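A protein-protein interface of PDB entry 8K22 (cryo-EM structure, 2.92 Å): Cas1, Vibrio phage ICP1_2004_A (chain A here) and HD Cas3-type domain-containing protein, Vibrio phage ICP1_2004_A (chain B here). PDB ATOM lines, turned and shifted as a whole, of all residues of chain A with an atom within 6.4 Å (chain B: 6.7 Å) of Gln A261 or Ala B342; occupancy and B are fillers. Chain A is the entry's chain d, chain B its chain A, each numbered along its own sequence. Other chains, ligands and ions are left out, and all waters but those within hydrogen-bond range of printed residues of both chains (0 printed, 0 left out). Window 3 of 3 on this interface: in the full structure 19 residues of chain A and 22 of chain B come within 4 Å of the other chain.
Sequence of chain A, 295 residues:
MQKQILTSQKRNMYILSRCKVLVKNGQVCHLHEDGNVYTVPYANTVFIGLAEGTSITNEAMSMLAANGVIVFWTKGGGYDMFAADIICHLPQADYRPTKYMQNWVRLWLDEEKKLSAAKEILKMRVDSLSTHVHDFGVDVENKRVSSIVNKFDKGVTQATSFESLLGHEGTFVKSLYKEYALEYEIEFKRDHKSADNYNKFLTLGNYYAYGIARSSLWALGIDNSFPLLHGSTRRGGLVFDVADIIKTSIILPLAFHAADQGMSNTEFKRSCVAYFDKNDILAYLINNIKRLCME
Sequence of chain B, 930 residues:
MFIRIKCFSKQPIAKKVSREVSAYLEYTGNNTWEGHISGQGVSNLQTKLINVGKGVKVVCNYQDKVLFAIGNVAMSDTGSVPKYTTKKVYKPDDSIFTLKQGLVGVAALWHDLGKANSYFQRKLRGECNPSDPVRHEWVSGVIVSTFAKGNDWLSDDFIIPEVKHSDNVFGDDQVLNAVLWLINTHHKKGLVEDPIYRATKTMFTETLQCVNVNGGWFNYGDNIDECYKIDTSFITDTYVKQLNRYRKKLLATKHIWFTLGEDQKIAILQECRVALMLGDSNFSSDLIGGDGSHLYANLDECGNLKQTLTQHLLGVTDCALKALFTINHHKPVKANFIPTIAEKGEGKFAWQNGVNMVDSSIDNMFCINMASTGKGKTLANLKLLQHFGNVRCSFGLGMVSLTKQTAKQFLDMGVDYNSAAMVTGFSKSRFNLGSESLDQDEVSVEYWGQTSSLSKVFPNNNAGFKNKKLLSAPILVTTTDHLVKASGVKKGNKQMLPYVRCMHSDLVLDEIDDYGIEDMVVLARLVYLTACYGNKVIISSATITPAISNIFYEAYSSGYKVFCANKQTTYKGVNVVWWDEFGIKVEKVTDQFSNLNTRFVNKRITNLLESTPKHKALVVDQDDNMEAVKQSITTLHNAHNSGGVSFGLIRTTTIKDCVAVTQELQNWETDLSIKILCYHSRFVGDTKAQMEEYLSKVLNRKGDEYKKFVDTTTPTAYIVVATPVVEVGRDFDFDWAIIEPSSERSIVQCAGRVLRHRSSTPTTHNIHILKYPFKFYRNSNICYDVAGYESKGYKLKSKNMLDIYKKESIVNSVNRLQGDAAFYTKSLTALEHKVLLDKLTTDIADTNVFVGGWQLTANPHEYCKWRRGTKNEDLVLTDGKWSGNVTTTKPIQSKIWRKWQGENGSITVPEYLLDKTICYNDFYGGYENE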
ATOM      1  N   TYR A 198      29.115   7.140  30.176  1.00  0.00           N
ATOM      2  CA  TYR A 198      28.549   6.340  31.263  1.00  0.00           C
ATOM      3  C   TYR A 198      28.065   7.222  32.411  1.00  0.00           C
ATOM      4  O   TYR A 198      27.206   6.803  33.191  1.00  0.00           O
ATOM      5  CB  TYR A 198      29.595   5.346  31.773  1.00  0.00           C
ATOM      6  CG  TYR A 198      30.017   4.304  30.759  1.00  0.00           C
ATOM      7  CD1 TYR A 198      31.084   4.542  29.894  1.00  0.00           C
ATOM      8  CD2 TYR A 198      29.376   3.077  30.682  1.00  0.00           C
ATOM      9  CE1 TYR A 198      31.489   3.593  28.967  1.00  0.00           C
ATOM     10  CE2 TYR A 198      29.771   2.122  29.755  1.00  0.00           C
ATOM     11  CZ  TYR A 198      30.830   2.386  28.902  1.00  0.00           C
ATOM     12  OH  TYR A 198      31.231   1.442  27.981  1.00  0.00           O
ATOM     13  N   LEU A 254      20.897   0.011  31.696  1.00  0.00           N
ATOM     14  CA  LEU A 254      20.481   0.652  30.451  1.00  0.00           C
ATOM     15  C   LEU A 254      21.407   1.805  30.089  1.00  0.00           C
ATOM     16  O   LEU A 254      21.720   2.005  28.910  1.00  0.00           O
ATOM     17  CB  LEU A 254      19.039   1.140  30.565  1.00  0.00           C
ATOM     18  CG  LEU A 254      18.207   1.311  29.298  1.00  0.00           C
ATOM     19  CD1 LEU A 254      18.443   0.167  28.333  1.00  0.00           C
ATOM     20  CD2 LEU A 254      16.739   1.402  29.667  1.00  0.00           C
ATOM     21  N   PHE A 256      24.617   1.975  30.962  1.00  0.00           N
ATOM     22  CA  PHE A 256      25.868   1.365  30.528  1.00  0.00           C
ATOM     23  C   PHE A 256      25.749   0.753  29.138  1.00  0.00           C
ATOM     24  O   PHE A 256      26.688   0.853  28.341  1.00  0.00           O
ATOM     25  CB  PHE A 256      26.321   0.320  31.543  1.00  0.00           C
ATOM     26  CG  PHE A 256      27.349   0.831  32.506  1.00  0.00           C
ATOM     27  CD1 PHE A 256      27.125   1.996  33.219  1.00  0.00           C
ATOM     28  CD2 PHE A 256      28.540   0.152  32.693  1.00  0.00           C
ATOM     29  CE1 PHE A 256      28.073   2.473  34.103  1.00  0.00           C
ATOM     30  CE2 PHE A 256      29.489   0.621  33.576  1.00  0.00           C
ATOM     31  CZ  PHE A 256      29.254   1.782  34.279  1.00  0.00           C
ATOM     32  N   HIS A 257      24.598   0.155  28.815  1.00  0.00           N
ATOM     33  CA  HIS A 257      24.386  -0.371  27.471  1.00  0.00           C
ATOM     34  C   HIS A 257      24.316   0.748  26.440  1.00  0.00           C
ATOM     35  O   HIS A 257      24.835   0.603  25.328  1.00  0.00           O
ATOM     36  CB  HIS A 257      23.113  -1.215  27.434  1.00  0.00           C
ATOM     37  CG  HIS A 257      22.977  -2.042  26.196  1.00  0.00           C
ATOM     38  ND1 HIS A 257      21.825  -2.069  25.440  1.00  0.00           N
ATOM     39  CD2 HIS A 257      23.853  -2.866  25.576  1.00  0.00           C
ATOM     40  CE1 HIS A 257      21.997  -2.878  24.410  1.00  0.00           C
ATOM     41  NE2 HIS A 257      23.218  -3.374  24.469  1.00  0.00           N
ATOM     42  N   ALA A 258      23.693   1.875  26.796  1.00  0.00           N
ATOM     43  CA  ALA A 258      23.601   2.999  25.871  1.00  0.00           C
ATOM     44  C   ALA A 258      24.954   3.671  25.677  1.00  0.00           C
ATOM     45  O   ALA A 258      25.265   4.144  24.577  1.00  0.00           O
ATOM     46  CB  ALA A 258      22.565   4.005  26.371  1.00  0.00           C
ATOM     47  N   ALA A 259      25.774   3.717  26.722  1.00  0.00           N
ATOM     48  CA  ALA A 259      27.119   4.259  26.608  1.00  0.00           C
ATOM     49  C   ALA A 259      28.098   3.270  26.000  1.00  0.00           C
ATOM     50  O   ALA A 259      29.210   3.666  25.640  1.00  0.00           O
ATOM     51  CB  ALA A 259      27.629   4.707  27.979  1.00  0.00           C
ATOM     52  N   ASP A 260      27.720   1.998  25.892  1.00  0.00           N
ATOM     53  CA  ASP A 260      28.551   1.004  25.229  1.00  0.00           C
ATOM     54  C   ASP A 260      28.238   0.968  23.734  1.00  0.00           C
ATOM     55  O   ASP A 260      29.158   0.946  22.910  1.00  0.00           O
ATOM     56  CB  ASP A 260      28.320  -0.365  25.892  1.00  0.00           C
ATOM     57  CG  ASP A 260      29.047  -1.526  25.204  1.00  0.00           C
ATOM     58  OD1 ASP A 260      30.030  -1.316  24.463  1.00  0.00           O
ATOM     59  OD2 ASP A 260      28.709  -2.686  25.525  1.00  0.00           O
ATOM     60  N   GLN A 261      26.952   0.977  23.366  1.00  0.00           N
ATOM     61  CA  GLN A 261      26.574   1.011  21.957  1.00  0.00           C
ATOM     62  C   GLN A 261      26.818   2.374  21.311  1.00  0.00           C
ATOM     63  O   GLN A 261      27.128   2.428  20.116  1.00  0.00           O
ATOM     64  CB  GLN A 261      25.113   0.563  21.794  1.00  0.00           C
ATOM     65  CG  GLN A 261      24.050   1.535  22.286  1.00  0.00           C
ATOM     66  CD  GLN A 261      22.717   0.870  22.551  1.00  0.00           C
ATOM     67  OE1 GLN A 261      22.469  -0.253  22.109  1.00  0.00           O
ATOM     68  NE2 GLN A 261      21.840   1.569  23.262  1.00  0.00           N
ATOM     69  N   GLY A 262      26.697   3.462  22.066  1.00  0.00           N
ATOM     70  CA  GLY A 262      27.206   4.766  21.672  1.00  0.00           C
ATOM     71  C   GLY A 262      26.593   5.493  20.490  1.00  0.00           C
ATOM     72  O   GLY A 262      27.330   6.085  19.692  1.00  0.00           O
ATOM     73  N   MET A 263      25.271   5.471  20.351  1.00  0.00           N
ATOM     74  CA  MET A 263      24.600   6.498  19.565  1.00  0.00           C
ATOM     75  C   MET A 263      24.174   7.632  20.500  1.00  0.00           C
ATOM     76  O   MET A 263      24.607   7.709  21.652  1.00  0.00           O
ATOM     77  CB  MET A 263      23.439   5.925  18.749  1.00  0.00           C
ATOM     78  CG  MET A 263      23.723   4.608  18.041  1.00  0.00           C
ATOM     79  SD  MET A 263      24.041   3.195  19.100  1.00  0.00           S
ATOM     80  CE  MET A 263      24.116   1.880  17.888  1.00  0.00           C
ATOM     81  N   GLU A 267      18.257   7.725  21.569  1.00  0.00           N
ATOM     82  CA  GLU A 267      18.045   6.289  21.726  1.00  0.00           C
ATOM     83  C   GLU A 267      17.948   5.917  23.199  1.00  0.00           C
ATOM     84  O   GLU A 267      17.231   4.981  23.559  1.00  0.00           O
ATOM     85  CB  GLU A 267      19.152   5.471  21.051  1.00  0.00           C
ATOM     86  CG  GLU A 267      20.544   5.683  21.614  1.00  0.00           C
ATOM     87  CD  GLU A 267      21.473   4.506  21.401  1.00  0.00           C
ATOM     88  OE1 GLU A 267      22.685   4.659  21.666  1.00  0.00           O
ATOM     89  OE2 GLU A 267      20.998   3.435  20.971  1.00  0.00           O
ATOM     90  N   PHE A 268      18.621   6.671  24.076  1.00  0.00           N
ATOM     91  CA  PHE A 268      18.502   6.402  25.503  1.00  0.00           C
ATOM     92  C   PHE A 268      17.158   6.863  26.045  1.00  0.00           C
ATOM     93  O   PHE A 268      16.574   6.185  26.901  1.00  0.00           O
ATOM     94  CB  PHE A 268      19.629   7.059  26.288  1.00  0.00           C
ATOM     95  CG  PHE A 268      19.749   6.539  27.685  1.00  0.00           C
ATOM     96  CD1 PHE A 268      19.417   5.224  27.982  1.00  0.00           C
ATOM     97  CD2 PHE A 268      20.111   7.379  28.716  1.00  0.00           C
ATOM     98  CE1 PHE A 268      19.495   4.752  29.273  1.00  0.00           C
ATOM     99  CE2 PHE A 268      20.183   6.910  30.002  1.00  0.00           C
ATOM    100  CZ  PHE A 268      19.876   5.600  30.284  1.00  0.00           C
ATOM    101  N   SER A 271      14.791   4.221  24.808  1.00  0.00           N
ATOM    102  CA  SER A 271      14.984   2.969  25.531  1.00  0.00           C
ATOM    103  C   SER A 271      14.406   3.045  26.938  1.00  0.00           C
ATOM    104  O   SER A 271      13.872   2.050  27.446  1.00  0.00           O
ATOM    105  CB  SER A 271      16.469   2.618  25.578  1.00  0.00           C
ATOM    106  OG  SER A 271      17.079   3.165  26.732  1.00  0.00           O
ATOM    107  N   PHE B 337      24.020   8.351   7.392  1.00  0.00           N
ATOM    108  CA  PHE B 337      24.375   7.604   8.593  1.00  0.00           C
ATOM    109  C   PHE B 337      24.842   6.233   8.137  1.00  0.00           C
ATOM    110  O   PHE B 337      24.029   5.359   7.838  1.00  0.00           O
ATOM    111  CB  PHE B 337      23.190   7.500   9.544  1.00  0.00           C
ATOM    112  CG  PHE B 337      23.525   6.870  10.865  1.00  0.00           C
ATOM    113  CD1 PHE B 337      24.047   7.634  11.894  1.00  0.00           C
ATOM    114  CD2 PHE B 337      23.308   5.517  11.080  1.00  0.00           C
ATOM    115  CE1 PHE B 337      24.357   7.060  13.112  1.00  0.00           C
ATOM    116  CE2 PHE B 337      23.614   4.938  12.294  1.00  0.00           C
ATOM    117  CZ  PHE B 337      24.139   5.710  13.311  1.00  0.00           C
ATOM    118  N   ILE B 338      26.155   6.045   8.070  1.00  0.00           N
ATOM    119  CA  ILE B 338      26.731   4.784   7.617  1.00  0.00           C
ATOM    120  C   ILE B 338      26.471   3.710   8.667  1.00  0.00           C
ATOM    121  O   ILE B 338      26.919   3.841   9.815  1.00  0.00           O
ATOM    122  CB  ILE B 338      28.232   4.928   7.339  1.00  0.00           C
ATOM    123  CG1 ILE B 338      28.458   5.863   6.158  1.00  0.00           C
ATOM    124  CG2 ILE B 338      28.840   3.578   7.052  1.00  0.00           C
ATOM    125  CD1 ILE B 338      28.963   7.229   6.551  1.00  0.00           C
ATOM    126  N   PRO B 339      25.757   2.637   8.321  1.00  0.00           N
ATOM    127  CA  PRO B 339      25.410   1.635   9.334  1.00  0.00           C
ATOM    128  C   PRO B 339      26.508   0.626   9.595  1.00  0.00           C
ATOM    129  O   PRO B 339      26.393  -0.144  10.557  1.00  0.00           O
ATOM    130  CB  PRO B 339      24.164   0.950   8.745  1.00  0.00           C
ATOM    131  CG  PRO B 339      23.832   1.716   7.478  1.00  0.00           C
ATOM    132  CD  PRO B 339      25.099   2.358   7.039  1.00  0.00           C
ATOM    133  N   THR B 340      27.556   0.593   8.775  1.00  0.00           N
ATOM    134  CA  THR B 340      28.672  -0.316   9.001  1.00  0.00           C
ATOM    135  C   THR B 340      29.758   0.300   9.867  1.00  0.00           C
ATOM    136  O   THR B 340      30.819  -0.311  10.034  1.00  0.00           O
ATOM    137  CB  THR B 340      29.275  -0.765   7.669  1.00  0.00           C
ATOM    138  OG1 THR B 340      29.740   0.378   6.947  1.00  0.00           O
ATOM    139  CG2 THR B 340      28.235  -1.489   6.833  1.00  0.00           C
ATOM    140  N   ILE B 341      29.527   1.492  10.405  1.00  0.00           N
ATOM    141  CA  ILE B 341      30.482   2.134  11.298  1.00  0.00           C
ATOM    142  C   ILE B 341      30.078   1.964  12.758  1.00  0.00           C
ATOM    143  O   ILE B 341      30.906   1.604  13.600  1.00  0.00           O
ATOM    144  CB  ILE B 341      30.617   3.622  10.910  1.00  0.00           C
ATOM    145  CG1 ILE B 341      31.536   3.777   9.699  1.00  0.00           C
ATOM    146  CG2 ILE B 341      31.105   4.469  12.076  1.00  0.00           C
ATOM    147  CD1 ILE B 341      33.006   3.621  10.008  1.00  0.00           C
ATOM    148  N   ALA B 342      28.791   2.162  13.058  1.00  0.00           N
ATOM    149  CA  ALA B 342      28.300   2.344  14.419  1.00  0.00           C
ATOM    150  C   ALA B 342      28.382   1.093  15.285  1.00  0.00           C
ATOM    151  O   ALA B 342      28.208   1.202  16.504  1.00  0.00           O
ATOM    152  CB  ALA B 342      26.854   2.840  14.384  1.00  0.00           C
ATOM    153  N   GLU B 343      28.636  -0.079  14.712  1.00  0.00           N
ATOM    154  CA  GLU B 343      28.744  -1.259  15.552  1.00  0.00           C
ATOM    155  C   GLU B 343      30.136  -1.343  16.175  1.00  0.00           C
ATOM    156  O   GLU B 343      30.996  -0.480  15.979  1.00  0.00           O
ATOM    157  CB  GLU B 343      28.439  -2.534  14.763  1.00  0.00           C
ATOM    158  CG  GLU B 343      29.396  -2.872  13.618  1.00  0.00           C
ATOM    159  CD  GLU B 343      29.119  -2.133  12.322  1.00  0.00           C
ATOM    160  OE1 GLU B 343      28.455  -1.076  12.344  1.00  0.00           O
ATOM    161  OE2 GLU B 343      29.561  -2.632  11.267  1.00  0.00           O
ATOM    162  N   LYS B 344      30.342  -2.403  16.949  1.00  0.00           N
ATOM    163  CA  LYS B 344      31.581  -2.577  17.692  1.00  0.00           C
ATOM    164  C   LYS B 344      32.730  -2.950  16.765  1.00  0.00           C
ATOM    165  O   LYS B 344      32.553  -3.695  15.797  1.00  0.00           O
ATOM    166  CB  LYS B 344      31.413  -3.667  18.752  1.00  0.00           C
ATOM    167  CG  LYS B 344      31.060  -3.177  20.148  1.00  0.00           C
ATOM    168  CD  LYS B 344      29.619  -2.688  20.201  1.00  0.00           C
ATOM    169  CE  LYS B 344      29.087  -2.631  21.617  1.00  0.00           C
ATOM    170  NZ  LYS B 344      27.657  -2.219  21.683  1.00  0.00           N
ATOM    171  N   ASN B 356      32.918   5.710  22.123  1.00  0.00           N
ATOM    172  CA  ASN B 356      31.909   5.618  23.172  1.00  0.00           C
ATOM    173  C   ASN B 356      32.379   6.237  24.485  1.00  0.00           C
ATOM    174  O   ASN B 356      31.637   6.215  25.473  1.00  0.00           O
ATOM    175  CB  ASN B 356      31.489   4.164  23.364  1.00  0.00           C
ATOM    176  CG  ASN B 356      31.247   3.448  22.049  1.00  0.00           C
ATOM    177  OD1 ASN B 356      32.134   3.322  21.213  1.00  0.00           O
ATOM    178  ND2 ASN B 356      30.030   2.955  21.870  1.00  0.00           N
ATOM    179  N   LYS B 383      34.477   7.087  12.335  1.00  0.00           N
ATOM    180  CA  LYS B 383      33.689   6.715  13.507  1.00  0.00           C
ATOM    181  C   LYS B 383      33.579   7.867  14.497  1.00  0.00           C
ATOM    182  O   LYS B 383      32.509   8.102  15.071  1.00  0.00           O
ATOM    183  CB  LYS B 383      34.308   5.491  14.179  1.00  0.00           C
ATOM    184  CG  LYS B 383      33.368   4.741  15.097  1.00  0.00           C
ATOM    185  CD  LYS B 383      33.892   3.349  15.391  1.00  0.00           C
ATOM    186  CE  LYS B 383      32.858   2.510  16.119  1.00  0.00           C
ATOM    187  NZ  LYS B 383      33.219   1.067  16.120  1.00  0.00           N
ATOM    188  N   GLN B 386      31.176  10.386  13.034  1.00  0.00           N
ATOM    189  CA  GLN B 386      29.797   9.928  13.099  1.00  0.00           C
ATOM    190  C   GLN B 386      29.285   9.773  14.525  1.00  0.00           C
ATOM    191  O   GLN B 386      28.070   9.647  14.718  1.00  0.00           O
ATOM    192  CB  GLN B 386      29.652   8.609  12.337  1.00  0.00           C
ATOM    193  CG  GLN B 386      28.266   8.378  11.768  1.00  0.00           C
ATOM    194  CD  GLN B 386      28.169   7.105  10.979  1.00  0.00           C
ATOM    195  OE1 GLN B 386      29.166   6.597  10.477  1.00  0.00           O
ATOM    196  NE2 GLN B 386      26.972   6.545  10.911  1.00  0.00           N
ATOM    197  N   HIS B 387      30.170   9.783  15.524  1.00  0.00           N
ATOM    198  CA  HIS B 387      29.706   9.739  16.906  1.00  0.00           C
ATOM    199  C   HIS B 387      28.955  11.008  17.300  1.00  0.00           C
ATOM    200  O   HIS B 387      28.035  10.950  18.122  1.00  0.00           O
ATOM    201  CB  HIS B 387      30.881   9.500  17.852  1.00  0.00           C
ATOM    202  CG  HIS B 387      30.492   9.484  19.295  1.00  0.00           C
ATOM    203  ND1 HIS B 387      29.638   8.541  19.823  1.00  0.00           N
ATOM    204  CD2 HIS B 387      30.832  10.300  20.320  1.00  0.00           C
ATOM    205  CE1 HIS B 387      29.467   8.777  21.111  1.00  0.00           C
ATOM    206  NE2 HIS B 387      30.184   9.836  21.439  1.00  0.00           N
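The side-chain carboxylate (OD1) of Asp A260 lies within salt-bridge range of the side-chain amino group (NZ) of Lys B344 (3.8 Å).
The side-chain amide nitrogen (ND2) of Asn B356 sits close to the backbone carbonyl oxygen (O) of Gln A261, at 3.4 Å.
The backbone carbonyl oxygen (O) of Asp A260 lies within hydrogen-bond range of the side-chain amide nitrogen (ND2) of Asn B356, 2.4 Å away.
ND2 of Asn B356 lies close to N of Gly A262 (3.4 Å).
O of Gly A262 lies within hydrogen-bond range of ND1 of His B387 (3.4 Å).
His A257 touches none of the printed residues of chain B.
Printed residues of chain B within 4 Å of Ala A259: Asn B356 (3.3 Å).
Of the printed residues of chain B, Asp A260 touches Lys B344 (3.3 Å) and Asn B356 (2.4 Å).
Of chain B, only Ala B342 (3.96 Å), Lys B344 (3.4 Å) and Asn B356 (3.3 Å) come within 4 Å of Gln A261.
Of the printed residues of chain B, Gly A262 touches Asn B356 and His B387.
Ala B342 touches just one residue of chain A: Gln A261 (3.96 Å).
Of the printed residues of chain A, Lys B344 touches Asp A260 and Gln A261.
Of the printed residues of chain A, His B387 touches Gly A262.
The nearest residue of chain B that does not touch Gln A261 is Glu B343 (6.1 Å).
The nearest printed residue of chain A that does not touch His B387 is Met A263 (5.0 Å).
Hydrophobic or aromatic side chains of chain B within 4 Å of the printed part of chain A: His B387.
Of the 13 printed residues of chain A, 4 touch a printed residue of chain B.
Among the printed residues, Asp or Glu carboxylates within 4 Å of a Lys or Arg side-chain nitrogen of the other chain: Asp A260 with Lys B344.
OE2 of Glu A267 is in hydrogen-bond range of NE2 of Gln A261, at 3.1 Å.
Asn B356 touches Ala A259 (CB to O, 3.3 Å).
O of Ala B342 touches O of Gln A261 (3.96 Å).
Gln A261 touches Lys B344 (CA to NZ, 3.4 Å).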
